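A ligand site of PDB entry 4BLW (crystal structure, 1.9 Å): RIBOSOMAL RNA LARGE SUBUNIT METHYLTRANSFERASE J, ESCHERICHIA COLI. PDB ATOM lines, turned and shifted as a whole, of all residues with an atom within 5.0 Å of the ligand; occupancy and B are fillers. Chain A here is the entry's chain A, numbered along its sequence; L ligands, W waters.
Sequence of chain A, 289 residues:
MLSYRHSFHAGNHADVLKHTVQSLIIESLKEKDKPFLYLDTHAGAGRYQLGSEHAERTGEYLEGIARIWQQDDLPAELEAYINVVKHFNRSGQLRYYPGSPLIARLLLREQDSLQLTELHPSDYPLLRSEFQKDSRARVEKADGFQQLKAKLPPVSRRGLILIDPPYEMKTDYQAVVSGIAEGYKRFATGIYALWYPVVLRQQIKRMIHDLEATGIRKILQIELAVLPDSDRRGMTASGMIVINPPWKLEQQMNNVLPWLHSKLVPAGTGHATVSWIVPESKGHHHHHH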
ATOM      1  N   LEU A   2     -26.152  16.892   7.901  1.00  0.00           N
ATOM      2  CA  LEU A   2     -25.317  17.984   8.377  1.00  0.00           C
ATOM      3  C   LEU A   2     -26.051  19.283   8.743  1.00  0.00           C
ATOM      4  O   LEU A   2     -25.641  20.368   8.330  1.00  0.00           O
ATOM      5  CB  LEU A   2     -24.272  18.305   7.308  1.00  0.00           C
ATOM      6  CG  LEU A   2     -23.368  17.109   6.982  1.00  0.00           C
ATOM      7  CD1 LEU A   2     -22.656  17.295   5.619  1.00  0.00           C
ATOM      8  CD2 LEU A   2     -22.367  16.869   8.107  1.00  0.00           C
ATOM      9  N   TYR A   4     -26.299  20.229  11.919  1.00  0.00           N
ATOM     10  CA  TYR A   4     -25.630  20.683  13.132  1.00  0.00           C
ATOM     11  C   TYR A   4     -24.726  21.869  12.862  1.00  0.00           C
ATOM     12  O   TYR A   4     -23.955  21.874  11.908  1.00  0.00           O
ATOM     13  CB  TYR A   4     -24.833  19.533  13.764  1.00  0.00           C
ATOM     14  CG  TYR A   4     -23.991  19.897  14.983  1.00  0.00           C
ATOM     15  CD1 TYR A   4     -22.701  20.398  14.841  1.00  0.00           C
ATOM     16  CD2 TYR A   4     -24.497  19.741  16.279  1.00  0.00           C
ATOM     17  CE1 TYR A   4     -21.926  20.726  15.949  1.00  0.00           C
ATOM     18  CE2 TYR A   4     -23.723  20.074  17.399  1.00  0.00           C
ATOM     19  CZ  TYR A   4     -22.443  20.563  17.224  1.00  0.00           C
ATOM     20  OH  TYR A   4     -21.676  20.898  18.313  1.00  0.00           O
ATOM     21  N   HIS A   6     -21.882  24.106  14.977  1.00  0.00           N
ATOM     22  CA  HIS A   6     -21.153  24.183  16.249  1.00  0.00           C
ATOM     23  C   HIS A   6     -21.216  25.559  16.895  1.00  0.00           C
ATOM     24  O   HIS A   6     -21.054  25.680  18.104  1.00  0.00           O
ATOM     25  CB  HIS A   6     -19.705  23.724  16.136  1.00  0.00           C
ATOM     26  CG  HIS A   6     -19.084  23.428  17.463  1.00  0.00           C
ATOM     27  ND1 HIS A   6     -19.573  22.454  18.306  1.00  0.00           N
ATOM     28  CD2 HIS A   6     -18.027  23.982  18.104  1.00  0.00           C
ATOM     29  CE1 HIS A   6     -18.841  22.402  19.407  1.00  0.00           C
ATOM     30  NE2 HIS A   6     -17.890  23.320  19.305  1.00  0.00           N
ATOM     31  N   ASP A  15     -16.833  22.231  25.389  1.00  0.00           N
ATOM     32  CA  ASP A  15     -15.652  22.699  24.680  1.00  0.00           C
ATOM     33  C   ASP A  15     -14.504  22.990  25.633  1.00  0.00           C
ATOM     34  O   ASP A  15     -13.350  22.661  25.351  1.00  0.00           O
ATOM     35  CB  ASP A  15     -15.977  23.950  23.849  1.00  0.00           C
ATOM     36  CG  ASP A  15     -16.425  23.618  22.415  1.00  0.00           C
ATOM     37  OD1 ASP A  15     -16.573  22.419  22.069  1.00  0.00           O
ATOM     38  OD2 ASP A  15     -16.625  24.578  21.637  1.00  0.00           O
ATOM     39  N   LYS A  18     -13.095  19.589  26.612  1.00  0.00           N
ATOM     40  CA  LYS A  18     -12.503  18.968  25.425  1.00  0.00           C
ATOM     41  C   LYS A  18     -11.149  19.600  25.080  1.00  0.00           C
ATOM     42  O   LYS A  18     -10.162  18.914  24.837  1.00  0.00           O
ATOM     43  CB  LYS A  18     -13.462  19.139  24.237  1.00  0.00           C
ATOM     44  CG  LYS A  18     -12.966  18.563  22.923  1.00  0.00           C
ATOM     45  CD  LYS A  18     -13.757  19.185  21.753  1.00  0.00           C
ATOM     46  CE  LYS A  18     -15.275  19.080  21.963  1.00  0.00           C
ATOM     47  NZ  LYS A  18     -16.053  19.784  20.884  1.00  0.00           N
ATOM     48  N   HIS A  19     -11.120  20.924  25.087  1.00  0.00           N
ATOM     49  CA  HIS A  19      -9.933  21.663  24.687  1.00  0.00           C
ATOM     50  C   HIS A  19      -8.882  21.704  25.779  1.00  0.00           C
ATOM     51  O   HIS A  19      -7.701  21.835  25.481  1.00  0.00           O
ATOM     52  CB  HIS A  19     -10.309  23.053  24.194  1.00  0.00           C
ATOM     53  CG  HIS A  19     -11.153  23.037  22.954  1.00  0.00           C
ATOM     54  ND1 HIS A  19     -12.052  24.034  22.644  1.00  0.00           N
ATOM     55  CD2 HIS A  19     -11.228  22.124  21.949  1.00  0.00           C
ATOM     56  CE1 HIS A  19     -12.646  23.746  21.494  1.00  0.00           C
ATOM     57  NE2 HIS A  19     -12.167  22.596  21.053  1.00  0.00           N
ATOM     58  N   ASP A  40      -7.672  15.574  13.131  1.00  0.00           N
ATOM     59  CA  ASP A  40      -8.952  16.042  13.657  1.00  0.00           C
ATOM     60  C   ASP A  40     -10.042  15.603  12.663  1.00  0.00           C
ATOM     61  O   ASP A  40     -10.171  16.171  11.596  1.00  0.00           O
ATOM     62  CB  ASP A  40      -8.894  17.562  13.767  1.00  0.00           C
ATOM     63  CG  ASP A  40      -9.967  18.158  14.665  1.00  0.00           C
ATOM     64  OD1 ASP A  40     -11.058  17.574  14.780  1.00  0.00           O
ATOM     65  OD2 ASP A  40      -9.713  19.229  15.252  1.00  0.00           O
ATOM     66  N   THR A  41     -10.814  14.575  13.019  1.00  0.00           N
ATOM     67  CA  THR A  41     -11.728  13.949  12.051  1.00  0.00           C
ATOM     68  C   THR A  41     -12.942  14.839  11.732  1.00  0.00           C
ATOM     69  O   THR A  41     -13.404  14.903  10.590  1.00  0.00           O
ATOM     70  CB  THR A  41     -12.225  12.582  12.554  1.00  0.00           C
ATOM     71  OG1 THR A  41     -12.919  12.761  13.792  1.00  0.00           O
ATOM     72  CG2 THR A  41     -11.036  11.587  12.767  1.00  0.00           C
ATOM     73  N   HIS A  42     -13.456  15.502  12.758  1.00  0.00           N
ATOM     74  CA  HIS A  42     -14.600  16.383  12.612  1.00  0.00           C
ATOM     75  C   HIS A  42     -14.173  17.772  13.055  1.00  0.00           C
ATOM     76  O   HIS A  42     -14.426  18.170  14.192  1.00  0.00           O
ATOM     77  CB  HIS A  42     -15.751  15.887  13.468  1.00  0.00           C
ATOM     78  CG  HIS A  42     -16.277  14.553  13.060  1.00  0.00           C
ATOM     79  ND1 HIS A  42     -15.516  13.399  13.096  1.00  0.00           N
ATOM     80  CD2 HIS A  42     -17.517  14.173  12.662  1.00  0.00           C
ATOM     81  CE1 HIS A  42     -16.249  12.379  12.720  1.00  0.00           C
ATOM     82  NE2 HIS A  42     -17.467  12.818  12.445  1.00  0.00           N
ATOM     83  N   ALA A  43     -13.541  18.513  12.155  1.00  0.00           N
ATOM     84  CA  ALA A  43     -12.755  19.659  12.533  1.00  0.00           C
ATOM     85  C   ALA A  43     -13.530  20.953  12.777  1.00  0.00           C
ATOM     86  O   ALA A  43     -13.053  21.840  13.474  1.00  0.00           O
ATOM     87  CB  ALA A  43     -11.635  19.890  11.516  1.00  0.00           C
ATOM     88  N   GLY A  44     -14.725  21.095  12.198  1.00  0.00           N
ATOM     89  CA  GLY A  44     -15.443  22.355  12.375  1.00  0.00           C
ATOM     90  C   GLY A  44     -14.909  23.481  11.502  1.00  0.00           C
ATOM     91  O   GLY A  44     -14.121  23.230  10.575  1.00  0.00           O
ATOM     92  N   TYR A  48     -14.993  30.542  15.924  1.00  0.00           N
ATOM     93  CA  TYR A  48     -16.401  30.822  16.059  1.00  0.00           C
ATOM     94  C   TYR A  48     -16.632  32.216  16.606  1.00  0.00           C
ATOM     95  O   TYR A  48     -15.893  32.673  17.468  1.00  0.00           O
ATOM     96  CB  TYR A  48     -17.071  29.765  16.929  1.00  0.00           C
ATOM     97  CG  TYR A  48     -16.909  28.396  16.339  1.00  0.00           C
ATOM     98  CD1 TYR A  48     -17.767  27.945  15.355  1.00  0.00           C
ATOM     99  CD2 TYR A  48     -15.865  27.571  16.722  1.00  0.00           C
ATOM    100  CE1 TYR A  48     -17.613  26.712  14.782  1.00  0.00           C
ATOM    101  CE2 TYR A  48     -15.692  26.324  16.148  1.00  0.00           C
ATOM    102  CZ  TYR A  48     -16.566  25.905  15.181  1.00  0.00           C
ATOM    103  OH  TYR A  48     -16.396  24.662  14.598  1.00  0.00           O
ATOM    104  N   GLY A  99     -11.603  26.916  17.729  1.00  0.00           N
ATOM    105  CA  GLY A  99     -11.935  25.510  17.728  1.00  0.00           C
ATOM    106  C   GLY A  99     -10.695  24.644  17.866  1.00  0.00           C
ATOM    107  O   GLY A  99      -9.559  25.148  17.873  1.00  0.00           O
ATOM    108  N   SER A 100     -10.916  23.342  17.984  1.00  0.00           N
ATOM    109  CA  SER A 100      -9.799  22.392  18.070  1.00  0.00           C
ATOM    110  C   SER A 100      -8.691  22.595  17.025  1.00  0.00           C
ATOM    111  O   SER A 100      -7.506  22.502  17.367  1.00  0.00           O
ATOM    112  CB  SER A 100     -10.303  20.928  18.103  1.00  0.00           C
ATOM    113  OG  SER A 100     -11.032  20.580  16.915  1.00  0.00           O
ATOM    114  N   PRO A 101      -9.046  22.879  15.762  1.00  0.00           N
ATOM    115  CA  PRO A 101      -7.932  23.059  14.808  1.00  0.00           C
ATOM    116  C   PRO A 101      -7.023  24.252  15.101  1.00  0.00           C
ATOM    117  O   PRO A 101      -5.822  24.145  14.846  1.00  0.00           O
ATOM    118  CB  PRO A 101      -8.654  23.242  13.457  1.00  0.00           C
ATOM    119  CG  PRO A 101      -9.964  22.604  13.624  1.00  0.00           C
ATOM    120  CD  PRO A 101     -10.348  22.893  15.066  1.00  0.00           C
ATOM    121  N   THR A 117     -10.442  17.352   8.614  1.00  0.00           N
ATOM    122  CA  THR A 117     -11.565  17.144   7.692  1.00  0.00           C
ATOM    123  C   THR A 117     -12.833  17.756   8.242  1.00  0.00           C
ATOM    124  O   THR A 117     -13.036  17.798   9.459  1.00  0.00           O
ATOM    125  CB  THR A 117     -11.805  15.639   7.386  1.00  0.00           C
ATOM    126  OG1 THR A 117     -11.676  14.873   8.586  1.00  0.00           O
ATOM    127  CG2 THR A 117     -10.795  15.109   6.355  1.00  0.00           C
ATOM    128  N   GLU A 118     -13.694  18.233   7.340  1.00  0.00           N
ATOM    129  CA  GLU A 118     -14.980  18.802   7.700  1.00  0.00           C
ATOM    130  C   GLU A 118     -15.877  18.681   6.465  1.00  0.00           C
ATOM    131  O   GLU A 118     -15.443  19.009   5.358  1.00  0.00           O
ATOM    132  CB  GLU A 118     -14.822  20.279   8.118  1.00  0.00           C
ATOM    133  CG  GLU A 118     -16.144  21.054   8.227  1.00  0.00           C
ATOM    134  CD  GLU A 118     -17.082  20.490   9.271  1.00  0.00           C
ATOM    135  OE1 GLU A 118     -16.621  20.247  10.397  1.00  0.00           O
ATOM    136  OE2 GLU A 118     -18.282  20.270   8.983  1.00  0.00           O
ATOM    137  N   LEU A 119     -17.084  18.168   6.638  1.00  0.00           N
ATOM    138  CA  LEU A 119     -17.999  17.969   5.506  1.00  0.00           C
ATOM    139  C   LEU A 119     -18.919  19.156   5.192  1.00  0.00           C
ATOM    140  O   LEU A 119     -19.391  19.298   4.058  1.00  0.00           O
ATOM    141  CB  LEU A 119     -18.824  16.699   5.728  1.00  0.00           C
ATOM    142  CG  LEU A 119     -18.110  15.367   5.404  1.00  0.00           C
ATOM    143  CD1 LEU A 119     -18.986  14.199   5.761  1.00  0.00           C
ATOM    144  CD2 LEU A 119     -17.819  15.336   3.909  1.00  0.00           C
ATOM    145  N   HIS A 120     -19.229  19.984   6.199  1.00  0.00           N
ATOM    146  CA  HIS A 120     -20.213  21.066   6.041  1.00  0.00           C
ATOM    147  C   HIS A 120     -19.795  22.153   5.041  1.00  0.00           C
ATOM    148  O   HIS A 120     -18.694  22.697   5.122  1.00  0.00           O
ATOM    149  CB  HIS A 120     -20.538  21.703   7.403  1.00  0.00           C
ATOM    150  CG  HIS A 120     -21.824  22.468   7.405  1.00  0.00           C
ATOM    151  ND1 HIS A 120     -21.925  23.757   6.920  1.00  0.00           N
ATOM    152  CD2 HIS A 120     -23.069  22.121   7.810  1.00  0.00           C
ATOM    153  CE1 HIS A 120     -23.171  24.176   7.044  1.00  0.00           C
ATOM    154  NE2 HIS A 120     -23.889  23.203   7.578  1.00  0.00           N
ATOM    155  N   ASP A 123     -18.755  25.409   6.802  1.00  0.00           N
ATOM    156  CA  ASP A 123     -17.592  25.307   7.689  1.00  0.00           C
ATOM    157  C   ASP A 123     -16.295  24.884   7.004  1.00  0.00           C
ATOM    158  O   ASP A 123     -15.225  25.359   7.365  1.00  0.00           O
ATOM    159  CB  ASP A 123     -17.894  24.369   8.868  1.00  0.00           C
ATOM    160  CG  ASP A 123     -19.020  24.865   9.716  1.00  0.00           C
ATOM    161  OD1 ASP A 123     -19.274  26.096   9.741  1.00  0.00           O
ATOM    162  OD2 ASP A 123     -19.664  24.021  10.382  1.00  0.00           O
ATOM    163  N   ALA A 142     -14.095  15.825   3.464  1.00  0.00           N
ATOM    164  CA  ALA A 142     -14.381  14.398   3.382  1.00  0.00           C
ATOM    165  C   ALA A 142     -14.828  13.823   4.721  1.00  0.00           C
ATOM    166  O   ALA A 142     -14.740  14.489   5.757  1.00  0.00           O
ATOM    167  CB  ALA A 142     -13.161  13.642   2.868  1.00  0.00           C
ATOM    168  N   ASP A 143     -15.303  12.591   4.701  1.00  0.00           N
ATOM    169  CA  ASP A 143     -15.761  11.920   5.909  1.00  0.00           C
ATOM    170  C   ASP A 143     -14.618  11.697   6.885  1.00  0.00           C
ATOM    171  O   ASP A 143     -13.618  11.060   6.541  1.00  0.00           O
ATOM    172  CB  ASP A 143     -16.431  10.589   5.568  1.00  0.00           C
ATOM    173  CG  ASP A 143     -16.913   9.846   6.793  1.00  0.00           C
ATOM    174  OD1 ASP A 143     -17.811  10.353   7.492  1.00  0.00           O
ATOM    175  OD2 ASP A 143     -16.389   8.738   7.070  1.00  0.00           O
ATOM    176  N   GLY A 144     -14.752  12.230   8.092  1.00  0.00           N
ATOM    177  CA  GLY A 144     -13.726  12.098   9.111  1.00  0.00           C
ATOM    178  C   GLY A 144     -13.440  10.654   9.505  1.00  0.00           C
ATOM    179  O   GLY A 144     -12.301  10.283   9.765  1.00  0.00           O
ATOM    180  N   PHE A 145     -14.476   9.836   9.596  1.00  0.00           N
ATOM    181  CA  PHE A 145     -14.284   8.460  10.027  1.00  0.00           C
ATOM    182  C   PHE A 145     -13.376   7.707   9.058  1.00  0.00           C
ATOM    183  O   PHE A 145     -12.593   6.850   9.461  1.00  0.00           O
ATOM    184  CB  PHE A 145     -15.618   7.729  10.205  1.00  0.00           C
ATOM    185  CG  PHE A 145     -16.443   8.273  11.340  1.00  0.00           C
ATOM    186  CD1 PHE A 145     -15.995   8.123  12.649  1.00  0.00           C
ATOM    187  CD2 PHE A 145     -17.652   8.905  11.108  1.00  0.00           C
ATOM    188  CE1 PHE A 145     -16.755   8.617  13.708  1.00  0.00           C
ATOM    189  CE2 PHE A 145     -18.403   9.404  12.165  1.00  0.00           C
ATOM    190  CZ  PHE A 145     -17.958   9.252  13.453  1.00  0.00           C
ATOM    191  N   LEU A 162      -8.080  13.354  17.421  1.00  0.00           N
ATOM    192  CA  LEU A 162      -9.283  13.844  18.071  1.00  0.00           C
ATOM    193  C   LEU A 162     -10.477  13.426  17.237  1.00  0.00           C
ATOM    194  O   LEU A 162     -10.539  13.695  16.050  1.00  0.00           O
ATOM    195  CB  LEU A 162      -9.261  15.379  18.234  1.00  0.00           C
ATOM    196  CG  LEU A 162     -10.549  15.952  18.811  1.00  0.00           C
ATOM    197  CD1 LEU A 162     -10.673  15.626  20.297  1.00  0.00           C
ATOM    198  CD2 LEU A 162     -10.654  17.481  18.615  1.00  0.00           C
ATOM    199  N   ASP A 164     -14.370  14.018  17.307  1.00  0.00           N
ATOM    200  CA  ASP A 164     -15.309  14.897  17.973  1.00  0.00           C
ATOM    201  C   ASP A 164     -16.583  15.100  17.141  1.00  0.00           C
ATOM    202  O   ASP A 164     -16.878  16.214  16.701  1.00  0.00           O
ATOM    203  CB  ASP A 164     -14.606  16.227  18.234  1.00  0.00           C
ATOM    204  CG  ASP A 164     -15.469  17.246  18.944  1.00  0.00           C
ATOM    205  OD1 ASP A 164     -16.409  16.866  19.648  1.00  0.00           O
ATOM    206  OD2 ASP A 164     -15.166  18.441  18.779  1.00  0.00           O
ATOM    207  N   PRO A 165     -17.332  14.009  16.903  1.00  0.00           N
ATOM    208  CA  PRO A 165     -18.546  14.174  16.080  1.00  0.00           C
ATOM    209  C   PRO A 165     -19.677  14.907  16.835  1.00  0.00           C
ATOM    210  O   PRO A 165     -19.604  15.079  18.050  1.00  0.00           O
ATOM    211  CB  PRO A 165     -18.933  12.727  15.737  1.00  0.00           C
ATOM    212  CG  PRO A 165     -18.338  11.886  16.848  1.00  0.00           C
ATOM    213  CD  PRO A 165     -17.126  12.616  17.357  1.00  0.00           C
ATOM    214  N   PRO A 166     -20.703  15.354  16.108  1.00  0.00           N
ATOM    215  CA  PRO A 166     -21.817  16.064  16.735  1.00  0.00           C
ATOM    216  C   PRO A 166     -22.881  15.091  17.243  1.00  0.00           C
ATOM    217  O   PRO A 166     -23.717  15.516  18.014  1.00  0.00           O
ATOM    218  CB  PRO A 166     -22.393  16.901  15.582  1.00  0.00           C
ATOM    219  CG  PRO A 166     -22.145  16.019  14.366  1.00  0.00           C
ATOM    220  CD  PRO A 166     -20.778  15.388  14.628  1.00  0.00           C
HETATM  221  N1  LIG L   1     -13.770  19.568  16.635  1.00  0.00           N
HETATM  222  C1  LIG L   1     -14.363  20.913  16.591  1.00  0.00           C
HETATM  223  C2  LIG L   1     -15.896  20.896  16.602  1.00  0.00           C
HETATM  224  C3  LIG L   1     -16.572  19.950  15.621  1.00  0.00           C
HETATM  225  S1  LIG L   1     -18.364  19.950  15.837  1.00  0.00           S
HETATM  226  C4  LIG L   1     -13.907  21.802  17.747  1.00  0.00           C
HETATM  227  O1  LIG L   1     -13.885  23.026  17.631  1.00  0.00           O
HETATM  228  O2  LIG L   1     -13.562  21.306  18.815  1.00  0.00           O
HETATM  229  C5  LIG L   1     -18.629  18.509  14.752  1.00  0.00           C
HETATM  230  C6  LIG L   1     -18.440  18.802  13.252  1.00  0.00           C
HETATM  231  O3  LIG L   1     -18.473  17.622  12.453  1.00  0.00           O
HETATM  232  C7  LIG L   1     -19.476  19.703  12.623  1.00  0.00           C
HETATM  233  O4  LIG L   1     -18.790  20.846  12.160  1.00  0.00           O
HETATM  234  C8  LIG L   1     -20.061  18.924  11.442  1.00  0.00           C
HETATM  235  O5  LIG L   1     -20.295  19.700  10.285  1.00  0.00           O
HETATM  236  C9  LIG L   1     -18.959  17.953  11.144  1.00  0.00           C
HETATM  237  N2  LIG L   1     -19.306  16.633  10.650  1.00  0.00           N
HETATM  238  C10 LIG L   1     -20.424  15.871  10.882  1.00  0.00           C
HETATM  239  N3  LIG L   1     -20.192  14.664  10.311  1.00  0.00           N
HETATM  240  C11 LIG L   1     -18.962  14.662   9.755  1.00  0.00           C
HETATM  241  C12 LIG L   1     -18.240  13.703   9.053  1.00  0.00           C
HETATM  242  N4  LIG L   1     -18.752  12.515   8.826  1.00  0.00           N
HETATM  243  N5  LIG L   1     -16.988  14.023   8.592  1.00  0.00           N
HETATM  244  C13 LIG L   1     -16.421  15.260   8.827  1.00  0.00           C
HETATM  245  N6  LIG L   1     -17.146  16.200   9.512  1.00  0.00           N
HETATM  246  C14 LIG L   1     -18.393  15.889   9.963  1.00  0.00           C
HETATM  247  O   HOH W   1     -23.337  14.409  10.688  1.00  0.00           O
HETATM  248  O   HOH W   2     -23.508  17.105  11.493  1.00  0.00           O
HETATM  249  O   HOH W   3     -13.661  24.120  14.905  1.00  0.00           O
HETATM  250  O   HOH W   4     -20.487  12.126  12.047  1.00  0.00           O
HETATM  251  O   HOH W   5     -19.960  23.219  12.665  1.00  0.00           O
HETATM  252  O   HOH W   6     -15.094  25.049  19.266  1.00  0.00           O
HETATM  253  O   HOH W   7     -23.022  19.549  10.429  1.00  0.00           O
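Leu 2 touches the ligand. Tyr 4 touches the ligand (CE1 to S1, 3.6 Å). O of Thr 41 touches C13 of the ligand, at 3.5 Å. Ala 43 touches the ligand. Gly 44 touches the ligand. CA of Gly 99 touches O1 of the ligand, at 3.2 Å. His 120 touches the ligand. OD2 of Asp 123 touches O4 of the ligand, at 3.7 Å. O of Ala 142 touches C13 of the ligand, at 3.6 Å. Pro 166 touches the ligand. Of the 28 residues printed, 21 come within 4 Å of the ligand.
Water W5 lies within hydrogen-bond range of the side-chain carboxylate of Asp 123, an oxygen (O4) of the ligand and the backbone NH of His 6. Water W7 lies within hydrogen-bond range of O5 of the ligand (2.7 Å), O of Tyr 4 (2.9 Å) and O of Leu 2 (3.5 Å). Water W6 lies within hydrogen-bond range of OD2 of Asp 15, O1 of the ligand and NE2 of His 6. Water W3 lies within hydrogen-bond range of O of Ala 43 (2.8 Å), OH of Tyr 48 (2.8 Å) and O1 of the ligand (2.9 Å). Water W4 lies within hydrogen-bond range of N3 of the ligand (3.1 Å) and NE2 of His 42 (3.1 Å).
The side-chain carboxylate (OD1) of Asp 40 lies within salt-bridge range of a nitrogen (N1) of the ligand (3.8 Å). An oxygen (O1) of the ligand is in hydrogen-bond range of the backbone NH of Ser 100. O of His 42 is in hydrogen-bond range of N1 of the ligand (2.9 Å). The side-chain hydroxyl of Ser 100 is in hydrogen-bond range of a nitrogen (N1) of the ligand, at 2.9 Å. The side-chain carboxylate (OD1) of Asp 143 sits at hydrogen-bond distance from a nitrogen (N4) of the ligand. A ring nitrogen (ND1) of His 6 sits close to a sulfur (S1) of the ligand. OE2 of Glu 118 sits at hydrogen-bond distance from O5 of the ligand. N6 of the ligand is in hydrogen-bond range of N of Leu 119, at 3.5 Å. The side-chain carboxylate (OD2) of Asp 164 is in salt-bridge range of a nitrogen (N1) of the ligand, at 2.8 Å. A ring nitrogen (NE2) of His 19 is in hydrogen-bond range of an oxygen (O2) of the ligand, at 2.9 Å. NZ of Lys 18 lies within salt-bridge range of O2 of the ligand (3.6 Å). A nitrogen (N5) of the ligand is in hydrogen-bond range of the backbone NH (N) of Gly 144, at 2.9 Å.
The side-chain hydroxyl (OG) of Ser 100 sits at hydrogen-bond distance from the side-chain carboxylate (OD2) of Asp 40 (2.5 Å). A ring nitrogen (NE2) of His 19 is in hydrogen-bond range of the backbone NH of Ser 100, 3.4 Å away. ND1 of His 19 lies close to O of Asp 15, 3.3 Å away. A ring nitrogen (ND1) of His 6 sits at hydrogen-bond distance from the side-chain hydroxyl (OH) of Tyr 4. NZ of Lys 18 is in salt-bridge range of OD2 of Asp 164 (2.6 Å). The side-chain hydroxyl (OG1) of Thr 41 is in hydrogen-bond range of a ring nitrogen (ND1) of His 42, 2.8 Å away. The side-chain carboxylate (OD2) of Asp 143 lies close to the backbone NH (N) of Phe 145. OE1 of Glu 118 is in hydrogen-bond range of N of Gly 44, at 2.7 Å.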
